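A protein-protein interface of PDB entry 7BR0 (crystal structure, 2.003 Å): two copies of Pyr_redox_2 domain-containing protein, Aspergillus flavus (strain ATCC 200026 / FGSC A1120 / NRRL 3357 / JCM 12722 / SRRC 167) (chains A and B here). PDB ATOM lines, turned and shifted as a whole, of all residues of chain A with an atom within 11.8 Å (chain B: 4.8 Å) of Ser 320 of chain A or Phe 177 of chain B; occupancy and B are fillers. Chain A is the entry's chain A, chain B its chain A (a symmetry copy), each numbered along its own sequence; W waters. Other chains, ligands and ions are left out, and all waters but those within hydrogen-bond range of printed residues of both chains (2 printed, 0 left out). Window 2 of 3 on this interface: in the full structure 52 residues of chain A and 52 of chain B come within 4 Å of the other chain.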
ATOM      1  N   ASP A  11     -26.334 -11.709   7.501  1.00  0.00           N
ATOM      2  CA  ASP A  11     -25.600 -11.854   8.751  1.00  0.00           C
ATOM      3  C   ASP A  11     -26.537 -11.569   9.923  1.00  0.00           C
ATOM      4  O   ASP A  11     -26.407 -12.170  10.989  1.00  0.00           O
ATOM      5  CB  ASP A  11     -24.383 -10.926   8.796  1.00  0.00           C
ATOM      6  CG  ASP A  11     -23.337 -11.281   7.750  1.00  0.00           C
ATOM      7  OD1 ASP A  11     -23.227 -12.472   7.390  1.00  0.00           O
ATOM      8  OD2 ASP A  11     -22.620 -10.369   7.294  1.00  0.00           O
ATOM      9  N   LEU A  28     -22.991  -2.055  11.450  1.00  0.00           N
ATOM     10  CA  LEU A  28     -22.799  -3.241  10.613  1.00  0.00           C
ATOM     11  C   LEU A  28     -22.294  -2.913   9.203  1.00  0.00           C
ATOM     12  O   LEU A  28     -21.556  -3.704   8.610  1.00  0.00           O
ATOM     13  CB  LEU A  28     -24.104  -4.043  10.510  1.00  0.00           C
ATOM     14  CG  LEU A  28     -24.569  -4.798  11.766  1.00  0.00           C
ATOM     15  CD1 LEU A  28     -25.876  -5.528  11.499  1.00  0.00           C
ATOM     16  CD2 LEU A  28     -23.513  -5.784  12.252  1.00  0.00           C
ATOM     17  N   ARG A  30     -20.210  -0.652   8.407  1.00  0.00           N
ATOM     18  CA  ARG A  30     -18.790  -0.319   8.507  1.00  0.00           C
ATOM     19  C   ARG A  30     -17.894  -1.551   8.396  1.00  0.00           C
ATOM     20  O   ARG A  30     -16.708  -1.434   8.086  1.00  0.00           O
ATOM     21  CB  ARG A  30     -18.504   0.405   9.828  1.00  0.00           C
ATOM     22  CG  ARG A  30     -19.117   1.801   9.930  1.00  0.00           C
ATOM     23  CD  ARG A  30     -18.514   2.756   8.903  1.00  0.00           C
ATOM     24  NE  ARG A  30     -17.060   2.843   9.025  1.00  0.00           N
ATOM     25  CZ  ARG A  30     -16.270   3.458   8.148  1.00  0.00           C
ATOM     26  NH1 ARG A  30     -16.787   4.040   7.073  1.00  0.00           N
ATOM     27  NH2 ARG A  30     -14.958   3.484   8.342  1.00  0.00           N
ATOM     28  N   THR A  31     -18.464  -2.724   8.660  1.00  0.00           N
ATOM     29  CA  THR A  31     -17.713  -3.973   8.645  1.00  0.00           C
ATOM     30  C   THR A  31     -18.191  -4.901   7.518  1.00  0.00           C
ATOM     31  O   THR A  31     -17.856  -6.087   7.497  1.00  0.00           O
ATOM     32  CB  THR A  31     -17.817  -4.693  10.008  1.00  0.00           C
ATOM     33  OG1 THR A  31     -19.192  -4.806  10.400  1.00  0.00           O
ATOM     34  CG2 THR A  31     -17.062  -3.906  11.079  1.00  0.00           C
ATOM     35  N   LEU A  32     -18.955  -4.336   6.583  1.00  0.00           N
ATOM     36  CA  LEU A  32     -19.462  -5.044   5.401  1.00  0.00           C
ATOM     37  C   LEU A  32     -20.420  -6.195   5.725  1.00  0.00           C
ATOM     38  O   LEU A  32     -20.737  -7.012   4.856  1.00  0.00           O
ATOM     39  CB  LEU A  32     -18.295  -5.574   4.552  1.00  0.00           C
ATOM     40  CG  LEU A  32     -17.437  -4.509   3.871  1.00  0.00           C
ATOM     41  CD1 LEU A  32     -16.197  -5.136   3.266  1.00  0.00           C
ATOM     42  CD2 LEU A  32     -18.234  -3.788   2.802  1.00  0.00           C
ATOM     43  N   HIS A  33     -20.908  -6.254   6.957  1.00  0.00           N
ATOM     44  CA  HIS A  33     -21.879  -7.279   7.312  1.00  0.00           C
ATOM     45  C   HIS A  33     -23.226  -6.952   6.679  1.00  0.00           C
ATOM     46  O   HIS A  33     -23.565  -5.782   6.474  1.00  0.00           O
ATOM     47  CB  HIS A  33     -22.001  -7.412   8.832  1.00  0.00           C
ATOM     48  CG  HIS A  33     -20.792  -8.024   9.473  1.00  0.00           C
ATOM     49  ND1 HIS A  33     -19.796  -7.271  10.056  1.00  0.00           N
ATOM     50  CD2 HIS A  33     -20.408  -9.317   9.594  1.00  0.00           C
ATOM     51  CE1 HIS A  33     -18.856  -8.075  10.523  1.00  0.00           C
ATOM     52  NE2 HIS A  33     -19.203  -9.322  10.256  1.00  0.00           N
ATOM     53  N   ARG A 115     -28.166 -15.246  10.176  1.00  0.00           N
ATOM     54  CA  ARG A 115     -27.274 -15.878  11.144  1.00  0.00           C
ATOM     55  C   ARG A 115     -27.555 -15.407  12.567  1.00  0.00           C
ATOM     56  O   ARG A 115     -27.337 -16.143  13.528  1.00  0.00           O
ATOM     57  CB  ARG A 115     -25.817 -15.588  10.790  1.00  0.00           C
ATOM     58  CG  ARG A 115     -25.402 -16.179   9.456  1.00  0.00           C
ATOM     59  CD  ARG A 115     -24.016 -15.739   9.023  1.00  0.00           C
ATOM     60  NE  ARG A 115     -23.837 -15.973   7.593  1.00  0.00           N
ATOM     61  CZ  ARG A 115     -23.534 -17.150   7.055  1.00  0.00           C
ATOM     62  NH1 ARG A 115     -23.355 -18.218   7.825  1.00  0.00           N
ATOM     63  NH2 ARG A 115     -23.406 -17.260   5.741  1.00  0.00           N
ATOM     64  N   LYS A 116     -28.020 -14.168  12.687  1.00  0.00           N
ATOM     65  CA  LYS A 116     -28.248 -13.540  13.983  1.00  0.00           C
ATOM     66  C   LYS A 116     -29.511 -12.695  13.944  1.00  0.00           C
ATOM     67  O   LYS A 116     -30.014 -12.370  12.871  1.00  0.00           O
ATOM     68  CB  LYS A 116     -27.058 -12.661  14.377  1.00  0.00           C
ATOM     69  CG  LYS A 116     -25.697 -13.338  14.277  1.00  0.00           C
ATOM     70  CD  LYS A 116     -25.515 -14.390  15.353  1.00  0.00           C
ATOM     71  CE  LYS A 116     -24.398 -15.363  14.992  1.00  0.00           C
ATOM     72  NZ  LYS A 116     -24.125 -16.328  16.094  1.00  0.00           N
ATOM     73  N   GLY A 308     -21.997  -5.075  17.692  1.00  0.00           N
ATOM     74  CA  GLY A 308     -20.700  -5.602  18.087  1.00  0.00           C
ATOM     75  C   GLY A 308     -20.724  -7.099  18.338  1.00  0.00           C
ATOM     76  O   GLY A 308     -19.797  -7.829  17.953  1.00  0.00           O
ATOM     77  N   GLY A 309     -21.786  -7.557  18.991  1.00  0.00           N
ATOM     78  CA  GLY A 309     -21.948  -8.966  19.289  1.00  0.00           C
ATOM     79  C   GLY A 309     -22.135  -9.773  18.020  1.00  0.00           C
ATOM     80  O   GLY A 309     -21.570 -10.857  17.870  1.00  0.00           O
ATOM     81  N   VAL A 310     -22.933  -9.236  17.103  1.00  0.00           N
ATOM     82  CA  VAL A 310     -23.147  -9.862  15.803  1.00  0.00           C
ATOM     83  C   VAL A 310     -21.829  -9.979  15.052  1.00  0.00           C
ATOM     84  O   VAL A 310     -21.498 -11.039  14.520  1.00  0.00           O
ATOM     85  CB  VAL A 310     -24.155  -9.061  14.951  1.00  0.00           C
ATOM     86  CG1 VAL A 310     -24.237  -9.611  13.523  1.00  0.00           C
ATOM     87  CG2 VAL A 310     -25.527  -9.076  15.604  1.00  0.00           C
ATOM     88  N   GLN A 311     -21.082  -8.879  15.013  1.00  0.00           N
ATOM     89  CA  GLN A 311     -19.815  -8.832  14.292  1.00  0.00           C
ATOM     90  C   GLN A 311     -18.850  -9.881  14.832  1.00  0.00           C
ATOM     91  O   GLN A 311     -18.246 -10.633  14.066  1.00  0.00           O
ATOM     92  CB  GLN A 311     -19.199  -7.430  14.389  1.00  0.00           C
ATOM     93  CG  GLN A 311     -19.949  -6.378  13.570  1.00  0.00           C
ATOM     94  CD  GLN A 311     -19.657  -4.949  13.998  1.00  0.00           C
ATOM     95  OE1 GLN A 311     -19.375  -4.679  15.163  1.00  0.00           O
ATOM     96  NE2 GLN A 311     -19.746  -4.024  13.055  1.00  0.00           N
ATOM     97  N   MET A 312     -18.730  -9.943  16.153  1.00  0.00           N
ATOM     98  CA  MET A 312     -17.788 -10.850  16.793  1.00  0.00           C
ATOM     99  C   MET A 312     -18.132 -12.305  16.489  1.00  0.00           C
ATOM    100  O   MET A 312     -17.250 -13.107  16.172  1.00  0.00           O
ATOM    101  CB  MET A 312     -17.766 -10.620  18.307  1.00  0.00           C
ATOM    102  CG  MET A 312     -16.715 -11.448  19.038  1.00  0.00           C
ATOM    103  SD  MET A 312     -16.647 -11.163  20.821  1.00  0.00           S
ATOM    104  CE  MET A 312     -16.204  -9.439  20.912  1.00  0.00           C
ATOM    105  N   GLN A 313     -19.413 -12.644  16.582  1.00  0.00           N
ATOM    106  CA  GLN A 313     -19.844 -14.024  16.388  1.00  0.00           C
ATOM    107  C   GLN A 313     -19.801 -14.426  14.916  1.00  0.00           C
ATOM    108  O   GLN A 313     -19.298 -15.497  14.575  1.00  0.00           O
ATOM    109  CB  GLN A 313     -21.252 -14.230  16.951  1.00  0.00           C
ATOM    110  CG  GLN A 313     -21.317 -14.108  18.466  1.00  0.00           C
ATOM    111  CD  GLN A 313     -22.663 -14.505  19.034  1.00  0.00           C
ATOM    112  OE1 GLN A 313     -23.551 -14.948  18.310  1.00  0.00           O
ATOM    113  NE2 GLN A 313     -22.818 -14.346  20.342  1.00  0.00           N
ATOM    114  N   VAL A 314     -20.316 -13.567  14.042  1.00  0.00           N
ATOM    115  CA  VAL A 314     -20.351 -13.883  12.619  1.00  0.00           C
ATOM    116  C   VAL A 314     -18.930 -13.995  12.073  1.00  0.00           C
ATOM    117  O   VAL A 314     -18.629 -14.924  11.321  1.00  0.00           O
ATOM    118  CB  VAL A 314     -21.156 -12.835  11.826  1.00  0.00           C
ATOM    119  CG1 VAL A 314     -21.020 -13.046  10.320  1.00  0.00           C
ATOM    120  CG2 VAL A 314     -22.626 -12.904  12.226  1.00  0.00           C
ATOM    121  N   ASN A 315     -18.055 -13.067  12.463  1.00  0.00           N
ATOM    122  CA  ASN A 315     -16.652 -13.122  12.048  1.00  0.00           C
ATOM    123  C   ASN A 315     -16.013 -14.456  12.421  1.00  0.00           C
ATOM    124  O   ASN A 315     -15.377 -15.107  11.587  1.00  0.00           O
ATOM    125  CB  ASN A 315     -15.841 -11.987  12.679  1.00  0.00           C
ATOM    126  CG  ASN A 315     -16.074 -10.645  12.010  1.00  0.00           C
ATOM    127  OD1 ASN A 315     -16.758 -10.546  10.989  1.00  0.00           O
ATOM    128  ND2 ASN A 315     -15.492  -9.597  12.584  1.00  0.00           N
ATOM    129  N   ALA A 316     -16.189 -14.861  13.675  1.00  0.00           N
ATOM    130  CA  ALA A 316     -15.591 -16.096  14.174  1.00  0.00           C
ATOM    131  C   ALA A 316     -16.126 -17.316  13.426  1.00  0.00           C
ATOM    132  O   ALA A 316     -15.369 -18.225  13.081  1.00  0.00           O
ATOM    133  CB  ALA A 316     -15.844 -16.237  15.668  1.00  0.00           C
ATOM    134  N   GLU A 317     -17.431 -17.328  13.169  1.00  0.00           N
ATOM    135  CA  GLU A 317     -18.066 -18.459  12.492  1.00  0.00           C
ATOM    136  C   GLU A 317     -17.556 -18.613  11.062  1.00  0.00           C
ATOM    137  O   GLU A 317     -17.325 -19.729  10.598  1.00  0.00           O
ATOM    138  CB  GLU A 317     -19.588 -18.296  12.504  1.00  0.00           C
ATOM    139  CG  GLU A 317     -20.209 -18.644  13.851  1.00  0.00           C
ATOM    140  CD  GLU A 317     -21.501 -17.888  14.136  1.00  0.00           C
ATOM    141  OE1 GLU A 317     -22.174 -17.422  13.185  1.00  0.00           O
ATOM    142  OE2 GLU A 317     -21.836 -17.758  15.327  1.00  0.00           O
ATOM    143  N   LYS A 318     -17.371 -17.493  10.369  1.00  0.00           N
ATOM    144  CA  LYS A 318     -16.845 -17.521   9.009  1.00  0.00           C
ATOM    145  C   LYS A 318     -15.372 -17.922   8.962  1.00  0.00           C
ATOM    146  O   LYS A 318     -15.003 -18.911   8.325  1.00  0.00           O
ATOM    147  CB  LYS A 318     -17.002 -16.154   8.338  1.00  0.00           C
ATOM    148  CG  LYS A 318     -18.438 -15.731   8.049  1.00  0.00           C
ATOM    149  CD  LYS A 318     -18.487 -14.462   7.187  1.00  0.00           C
ATOM    150  CE  LYS A 318     -17.859 -13.261   7.890  1.00  0.00           C
ATOM    151  NZ  LYS A 318     -17.921 -12.009   7.071  1.00  0.00           N
ATOM    152  N   TRP A 319     -14.530 -17.147   9.637  1.00  0.00           N
ATOM    153  CA  TRP A 319     -13.091 -17.205   9.387  1.00  0.00           C
ATOM    154  C   TRP A 319     -12.348 -18.286  10.172  1.00  0.00           C
ATOM    155  O   TRP A 319     -11.177 -18.549   9.898  1.00  0.00           O
ATOM    156  CB  TRP A 319     -12.467 -15.837   9.676  1.00  0.00           C
ATOM    157  CG  TRP A 319     -13.088 -14.724   8.873  1.00  0.00           C
ATOM    158  CD1 TRP A 319     -13.616 -13.559   9.356  1.00  0.00           C
ATOM    159  CD2 TRP A 319     -13.258 -14.678   7.449  1.00  0.00           C
ATOM    160  NE1 TRP A 319     -14.098 -12.792   8.322  1.00  0.00           N
ATOM    161  CE2 TRP A 319     -13.887 -13.454   7.141  1.00  0.00           C
ATOM    162  CE3 TRP A 319     -12.935 -15.551   6.404  1.00  0.00           C
ATOM    163  CZ2 TRP A 319     -14.202 -13.083   5.836  1.00  0.00           C
ATOM    164  CZ3 TRP A 319     -13.245 -15.179   5.106  1.00  0.00           C
ATOM    165  CH2 TRP A 319     -13.873 -13.956   4.834  1.00  0.00           C
ATOM    166  N   SER A 320     -13.014 -18.926  11.130  1.00  0.00           N
ATOM    167  CA  SER A 320     -12.392 -20.022  11.873  1.00  0.00           C
ATOM    168  C   SER A 320     -12.397 -21.319  11.058  1.00  0.00           C
ATOM    169  O   SER A 320     -11.760 -22.303  11.438  1.00  0.00           O
ATOM    170  CB  SER A 320     -13.103 -20.248  13.210  1.00  0.00           C
ATOM    171  OG  SER A 320     -14.435 -20.688  13.013  1.00  0.00           O
ATOM    172  N   GLN A 321     -13.119 -21.312   9.940  1.00  0.00           N
ATOM    173  CA  GLN A 321     -13.220 -22.479   9.066  1.00  0.00           C
ATOM    174  C   GLN A 321     -12.075 -22.513   8.043  1.00  0.00           C
ATOM    175  O   GLN A 321     -11.900 -21.559   7.284  1.00  0.00           O
ATOM    176  CB  GLN A 321     -14.568 -22.475   8.342  1.00  0.00           C
ATOM    177  CG  GLN A 321     -14.802 -23.684   7.450  1.00  0.00           C
ATOM    178  CD  GLN A 321     -16.172 -23.665   6.800  1.00  0.00           C
ATOM    179  OE1 GLN A 321     -16.973 -22.758   7.036  1.00  0.00           O
ATOM    180  NE2 GLN A 321     -16.449 -24.670   5.975  1.00  0.00           N
ATOM    181  N   PRO A 322     -11.299 -23.612   8.009  1.00  0.00           N
ATOM    182  CA  PRO A 322     -10.162 -23.671   7.077  1.00  0.00           C
ATOM    183  C   PRO A 322     -10.573 -23.691   5.605  1.00  0.00           C
ATOM    184  O   PRO A 322     -11.756 -23.863   5.307  1.00  0.00           O
ATOM    185  CB  PRO A 322      -9.464 -24.982   7.456  1.00  0.00           C
ATOM    186  CG  PRO A 322     -10.519 -25.806   8.093  1.00  0.00           C
ATOM    187  CD  PRO A 322     -11.410 -24.842   8.813  1.00  0.00           C
ATOM    188  N   ARG B 173      -6.411 -12.765  17.051  1.00  0.00           N
ATOM    189  CA  ARG B 173      -7.451 -13.474  16.312  1.00  0.00           C
ATOM    190  C   ARG B 173      -8.657 -12.574  16.054  1.00  0.00           C
ATOM    191  O   ARG B 173      -9.154 -12.480  14.932  1.00  0.00           O
ATOM    192  CB  ARG B 173      -7.866 -14.720  17.099  1.00  0.00           C
ATOM    193  CG  ARG B 173      -9.009 -15.531  16.514  1.00  0.00           C
ATOM    194  CD  ARG B 173      -9.189 -16.809  17.326  1.00  0.00           C
ATOM    195  NE  ARG B 173     -10.362 -17.583  16.926  1.00  0.00           N
ATOM    196  CZ  ARG B 173     -11.562 -17.491  17.494  1.00  0.00           C
ATOM    197  NH1 ARG B 173     -11.779 -16.654  18.500  1.00  0.00           N
ATOM    198  NH2 ARG B 173     -12.556 -18.245  17.049  1.00  0.00           N
ATOM    199  N   HIS B 174      -9.108 -11.905  17.110  1.00  0.00           N
ATOM    200  CA  HIS B 174     -10.253 -11.006  17.047  1.00  0.00           C
ATOM    201  C   HIS B 174     -10.058  -9.899  16.011  1.00  0.00           C
ATOM    202  O   HIS B 174     -10.945  -9.627  15.199  1.00  0.00           O
ATOM    203  CB  HIS B 174     -10.495 -10.394  18.432  1.00  0.00           C
ATOM    204  CG  HIS B 174     -11.616  -9.404  18.469  1.00  0.00           C
ATOM    205  ND1 HIS B 174     -12.936  -9.775  18.619  1.00  0.00           N
ATOM    206  CD2 HIS B 174     -11.613  -8.053  18.380  1.00  0.00           C
ATOM    207  CE1 HIS B 174     -13.696  -8.695  18.614  1.00  0.00           C
ATOM    208  NE2 HIS B 174     -12.917  -7.637  18.473  1.00  0.00           N
ATOM    209  N   LEU B 175      -8.892  -9.264  16.047  1.00  0.00           N
ATOM    210  CA  LEU B 175      -8.580  -8.177  15.127  1.00  0.00           C
ATOM    211  C   LEU B 175      -8.317  -8.712  13.715  1.00  0.00           C
ATOM    212  O   LEU B 175      -8.671  -8.069  12.724  1.00  0.00           O
ATOM    213  CB  LEU B 175      -7.373  -7.387  15.635  1.00  0.00           C
ATOM    214  CG  LEU B 175      -7.520  -6.725  17.012  1.00  0.00           C
ATOM    215  CD1 LEU B 175      -6.203  -6.102  17.462  1.00  0.00           C
ATOM    216  CD2 LEU B 175      -8.619  -5.681  17.012  1.00  0.00           C
ATOM    217  N   ALA B 176      -7.701  -9.888  13.618  1.00  0.00           N
ATOM    218  CA  ALA B 176      -7.414 -10.473  12.308  1.00  0.00           C
ATOM    219  C   ALA B 176      -8.708 -10.822  11.573  1.00  0.00           C
ATOM    220  O   ALA B 176      -8.797 -10.678  10.352  1.00  0.00           O
ATOM    221  CB  ALA B 176      -6.531 -11.705  12.452  1.00  0.00           C
ATOM    222  N   PHE B 177      -9.716 -11.265  12.319  1.00  0.00           N
ATOM    223  CA  PHE B 177     -11.007 -11.607  11.725  1.00  0.00           C
ATOM    224  C   PHE B 177     -11.755 -10.362  11.237  1.00  0.00           C
ATOM    225  O   PHE B 177     -12.485 -10.418  10.247  1.00  0.00           O
ATOM    226  CB  PHE B 177     -11.873 -12.376  12.726  1.00  0.00           C
ATOM    227  CG  PHE B 177     -11.465 -13.820  12.922  1.00  0.00           C
ATOM    228  CD1 PHE B 177     -10.391 -14.372  12.233  1.00  0.00           C
ATOM    229  CD2 PHE B 177     -12.174 -14.630  13.795  1.00  0.00           C
ATOM    230  CE1 PHE B 177     -10.033 -15.697  12.419  1.00  0.00           C
ATOM    231  CE2 PHE B 177     -11.819 -15.955  13.987  1.00  0.00           C
ATOM    232  CZ  PHE B 177     -10.747 -16.490  13.295  1.00  0.00           C
ATOM    233  N   GLN B 178     -11.583  -9.242  11.931  1.00  0.00           N
ATOM    234  CA  GLN B 178     -12.115  -7.972  11.452  1.00  0.00           C
ATOM    235  C   GLN B 178     -11.427  -7.571  10.148  1.00  0.00           C
ATOM    236  O   GLN B 178     -12.078  -7.187   9.178  1.00  0.00           O
ATOM    237  CB  GLN B 178     -11.920  -6.873  12.496  1.00  0.00           C
ATOM    238  CG  GLN B 178     -12.787  -7.012  13.735  1.00  0.00           C
ATOM    239  CD  GLN B 178     -12.491  -5.934  14.759  1.00  0.00           C
ATOM    240  OE1 GLN B 178     -11.330  -5.625  15.034  1.00  0.00           O
ATOM    241  NE2 GLN B 178     -13.536  -5.340  15.311  1.00  0.00           N
ATOM    242  N   ALA B 179     -10.102  -7.659  10.142  1.00  0.00           N
ATOM    243  CA  ALA B 179      -9.308  -7.267   8.985  1.00  0.00           C
ATOM    244  C   ALA B 179      -9.646  -8.131   7.772  1.00  0.00           C
ATOM    245  O   ALA B 179      -9.600  -7.659   6.638  1.00  0.00           O
ATOM    246  CB  ALA B 179      -7.828  -7.364   9.307  1.00  0.00           C
ATOM    247  N   ARG B 180      -9.997  -9.389   8.019  1.00  0.00           N
ATOM    248  CA  ARG B 180     -10.244 -10.341   6.940  1.00  0.00           C
ATOM    249  C   ARG B 180     -11.477  -9.955   6.121  1.00  0.00           C
ATOM    250  O   ARG B 180     -11.612 -10.358   4.962  1.00  0.00           O
ATOM    251  CB  ARG B 180     -10.399 -11.752   7.510  1.00  0.00           C
ATOM    252  CG  ARG B 180     -10.570 -12.854   6.467  1.00  0.00           C
ATOM    253  CD  ARG B 180      -9.374 -12.962   5.531  1.00  0.00           C
ATOM    254  NE  ARG B 180      -9.556 -14.039   4.559  1.00  0.00           N
ATOM    255  CZ  ARG B 180     -10.318 -13.950   3.472  1.00  0.00           C
ATOM    256  NH1 ARG B 180     -10.976 -12.827   3.199  1.00  0.00           N
ATOM    257  NH2 ARG B 180     -10.423 -14.989   2.654  1.00  0.00           N
ATOM    258  N   ASN B 181     -12.374  -9.175   6.715  1.00  0.00           N
ATOM    259  CA  ASN B 181     -13.528  -8.673   5.984  1.00  0.00           C
ATOM    260  C   ASN B 181     -13.131  -7.626   4.945  1.00  0.00           C
ATOM    261  O   ASN B 181     -13.912  -7.321   4.047  1.00  0.00           O
ATOM    262  CB  ASN B 181     -14.557  -8.077   6.947  1.00  0.00           C
ATOM    263  CG  ASN B 181     -15.152  -9.114   7.888  1.00  0.00           C
ATOM    264  OD1 ASN B 181     -15.203 -10.303   7.573  1.00  0.00           O
ATOM    265  ND2 ASN B 181     -15.605  -8.662   9.052  1.00  0.00           N
ATOM    266  N   LEU B 204      -4.473 -20.299  12.922  1.00  0.00           N
ATOM    267  CA  LEU B 204      -5.076 -19.522  11.841  1.00  0.00           C
ATOM    268  C   LEU B 204      -4.418 -19.777  10.486  1.00  0.00           C
ATOM    269  O   LEU B 204      -4.967 -19.408   9.446  1.00  0.00           O
ATOM    270  CB  LEU B 204      -5.011 -18.029  12.173  1.00  0.00           C
ATOM    271  CG  LEU B 204      -5.607 -17.635  13.530  1.00  0.00           C
ATOM    272  CD1 LEU B 204      -5.500 -16.136  13.741  1.00  0.00           C
ATOM    273  CD2 LEU B 204      -7.054 -18.085  13.645  1.00  0.00           C
ATOM    274  N   CYS B 207      -6.447 -21.359   7.983  1.00  0.00           N
ATOM    275  CA  CYS B 207      -7.540 -20.493   7.549  1.00  0.00           C
ATOM    276  C   CYS B 207      -7.046 -19.369   6.639  1.00  0.00           C
ATOM    277  O   CYS B 207      -7.821 -18.492   6.257  1.00  0.00           O
ATOM    278  CB  CYS B 207      -8.266 -19.908   8.761  1.00  0.00           C
ATOM    279  SG  CYS B 207      -8.960 -21.163   9.863  1.00  0.00           S
ATOM    280  N   PHE B 209      -4.310 -17.261   7.227  1.00  0.00           N
ATOM    281  CA  PHE B 209      -3.707 -16.120   7.907  1.00  0.00           C
ATOM    282  C   PHE B 209      -2.199 -16.292   8.015  1.00  0.00           C
ATOM    283  O   PHE B 209      -1.704 -17.401   8.220  1.00  0.00           O
ATOM    284  CB  PHE B 209      -4.322 -15.934   9.291  1.00  0.00           C
ATOM    285  CG  PHE B 209      -5.761 -15.508   9.256  1.00  0.00           C
ATOM    286  CD1 PHE B 209      -6.773 -16.444   9.137  1.00  0.00           C
ATOM    287  CD2 PHE B 209      -6.100 -14.168   9.332  1.00  0.00           C
ATOM    288  CE1 PHE B 209      -8.098 -16.052   9.098  1.00  0.00           C
ATOM    289  CE2 PHE B 209      -7.425 -13.769   9.295  1.00  0.00           C
ATOM    290  CZ  PHE B 209      -8.424 -14.714   9.175  1.00  0.00           C
HETATM  291  O   HOH W   1     -13.879 -10.164  15.070  1.00  0.00           O
HETATM  292  O   HOH W   2     -15.813  -6.963  11.713  1.00  0.00           O
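Ser 320 of chain A touches just these residues of chain B: Phe 177 and Cys 207.
Of chain A, only Asn 315, Ala 316, Trp 319 and Ser 320 come within 4 Å of Phe 177 of chain B.
His 174 of chain B touches just one residue of chain A: Met 312 (3.5 Å).
No residue of chain A comes within 4 Å of Ala 176 of chain B.
Of chain A, only Asn 315 comes within 4 Å of Gln 178 of chain B.
Ala 179 of chain B touches none of the printed residues of chain A.
Of chain A, only Thr 31, Leu 32, His 33, Asn 315, Lys 318 and Trp 319 come within 4 Å of Asn 181 of chain B.
Cys 207 of chain B touches just these residues of chain A: Trp 319 (3.4 Å), Ser 320 (3.4 Å), Gln 321 (3.9 Å) and Pro 322 (3.9 Å).
Printed residues of chain B within 4 Å of Lys 318 of chain A: Asn 181 (3.2 Å).
Printed residues of chain B within 4 Å of Trp 319 of chain A: Phe 177, Arg 180, Asn 181 and Cys 207.
Of the printed residues of chain B, Asn 315 of chain A touches Phe 177 (3.9 Å), Gln 178 (3.9 Å) and Asn 181 (2.9 Å).
Of the printed residues of chain B, Gln 321 of chain A touches Cys 207 (3.9 Å).
Arg 115 of chain A touches none of the printed residues of chain B.
The nearest printed residue of chain B that does not touch Ala 316 of chain A is Arg 173 of chain B (4.1 Å).
ND2 of Asn 315 of chain A sits close to O of Gln 311 of chain A, at 3.3 Å.
A ring nitrogen (NE2) of His 33 of chain A sits at hydrogen-bond distance from the side-chain amide oxygen (OD1) of Asn 315 of chain A (2.8 Å).
The side-chain hydroxyl (OG1) of Thr 31 of chain A is in hydrogen-bond range of a ring nitrogen (ND1) of His 33 of chain A, 2.6 Å away.
The side-chain hydroxyl (OG1) of Thr 31 of chain A sits at hydrogen-bond distance from the backbone carbonyl oxygen (O) of Leu 28 of chain A.
Water W2 lies within hydrogen-bond range of ND2 of Asn 315 of chain A (2.8 Å) and ND2 of Asn 181 of chain B (3.2 Å).
Water W1 lies within hydrogen-bond range of the backbone carbonyl oxygen of His 174 of chain B (3.0 Å) and the side-chain amide nitrogen of Asn 315 of chain A (3.0 Å).
Among the printed residues, pairs that only touch across the chains: Leu 32 of chain A with Asn 181 of chain B (3.3 Å), Trp 319 of chain A with Arg 180 of chain B (3.4 Å), Met 312 of chain A with His 174 of chain B (3.5 Å), His 33 of chain A with Asn 181 of chain B (3.6 Å), Ala 316 of chain A with Phe 177 of chain B (3.7 Å), Thr 31 of chain A with Asn 181 of chain B (3.8 Å), Gln 321 of chain A with Cys 207 of chain B (3.9 Å), Pro 322 of chain A with Cys 207 of chain B (3.9 Å), Asn 315 of chain A with Phe 177 of chain B (3.9 Å), Asn 315 of chain A with Gln 178 of chain B (3.9 Å) and Ser 320 of chain A with Phe 177 of chain B (3.97 Å).
The side-chain amino group of Lys 318 of chain A sits at hydrogen-bond distance from the side-chain amide oxygen of Asn 181 of chain B, at 3.2 Å.
O of Trp 319 of chain A sits close to SG of Cys 207 of chain B.
The side-chain amide oxygen (OD1) of Asn 315 of chain A lies within hydrogen-bond range of the side-chain amide nitrogen (ND2) of Asn 181 of chain B, at 2.9 Å.
The indole nitrogen (NE1) of Trp 319 of chain A lies close to the backbone carbonyl oxygen (O) of Phe 177 of chain B (3.5 Å).
The backbone carbonyl oxygen (O) of Ser 320 of chain A lies within hydrogen-bond range of the side-chain sulfur (SG) of Cys 207 of chain B.
The indole nitrogen (NE1) of Trp 319 of chain A lies within hydrogen-bond range of the side-chain amide oxygen (OD1) of Asn 181 of chain B (2.8 Å).
No position is printed for both chains.
Of the 12 printed residues of chain B, 6 touch a printed residue of chain A.
Printed residues of chain B that touch a printed residue of chain A: His 174, Phe 177, Gln 178, Arg 180, Asn 181 and Cys 207.
Of the 23 printed residues of chain A, 11 touch a printed residue of chain B.
Hydrophobic or aromatic side chains of chain A within 4 Å of the printed part of chain B: Leu 32, His 33, Met 312 and Trp 319.
Along chain A the printed residues that touch a printed residue of chain B span positions 31 to 322.
Among the printed residues, 17 pairs touch across the chains.
Among the printed residues, no Asp or Glu carboxylate lies within 4 Å of a Lys or Arg side-chain nitrogen of the other chain.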
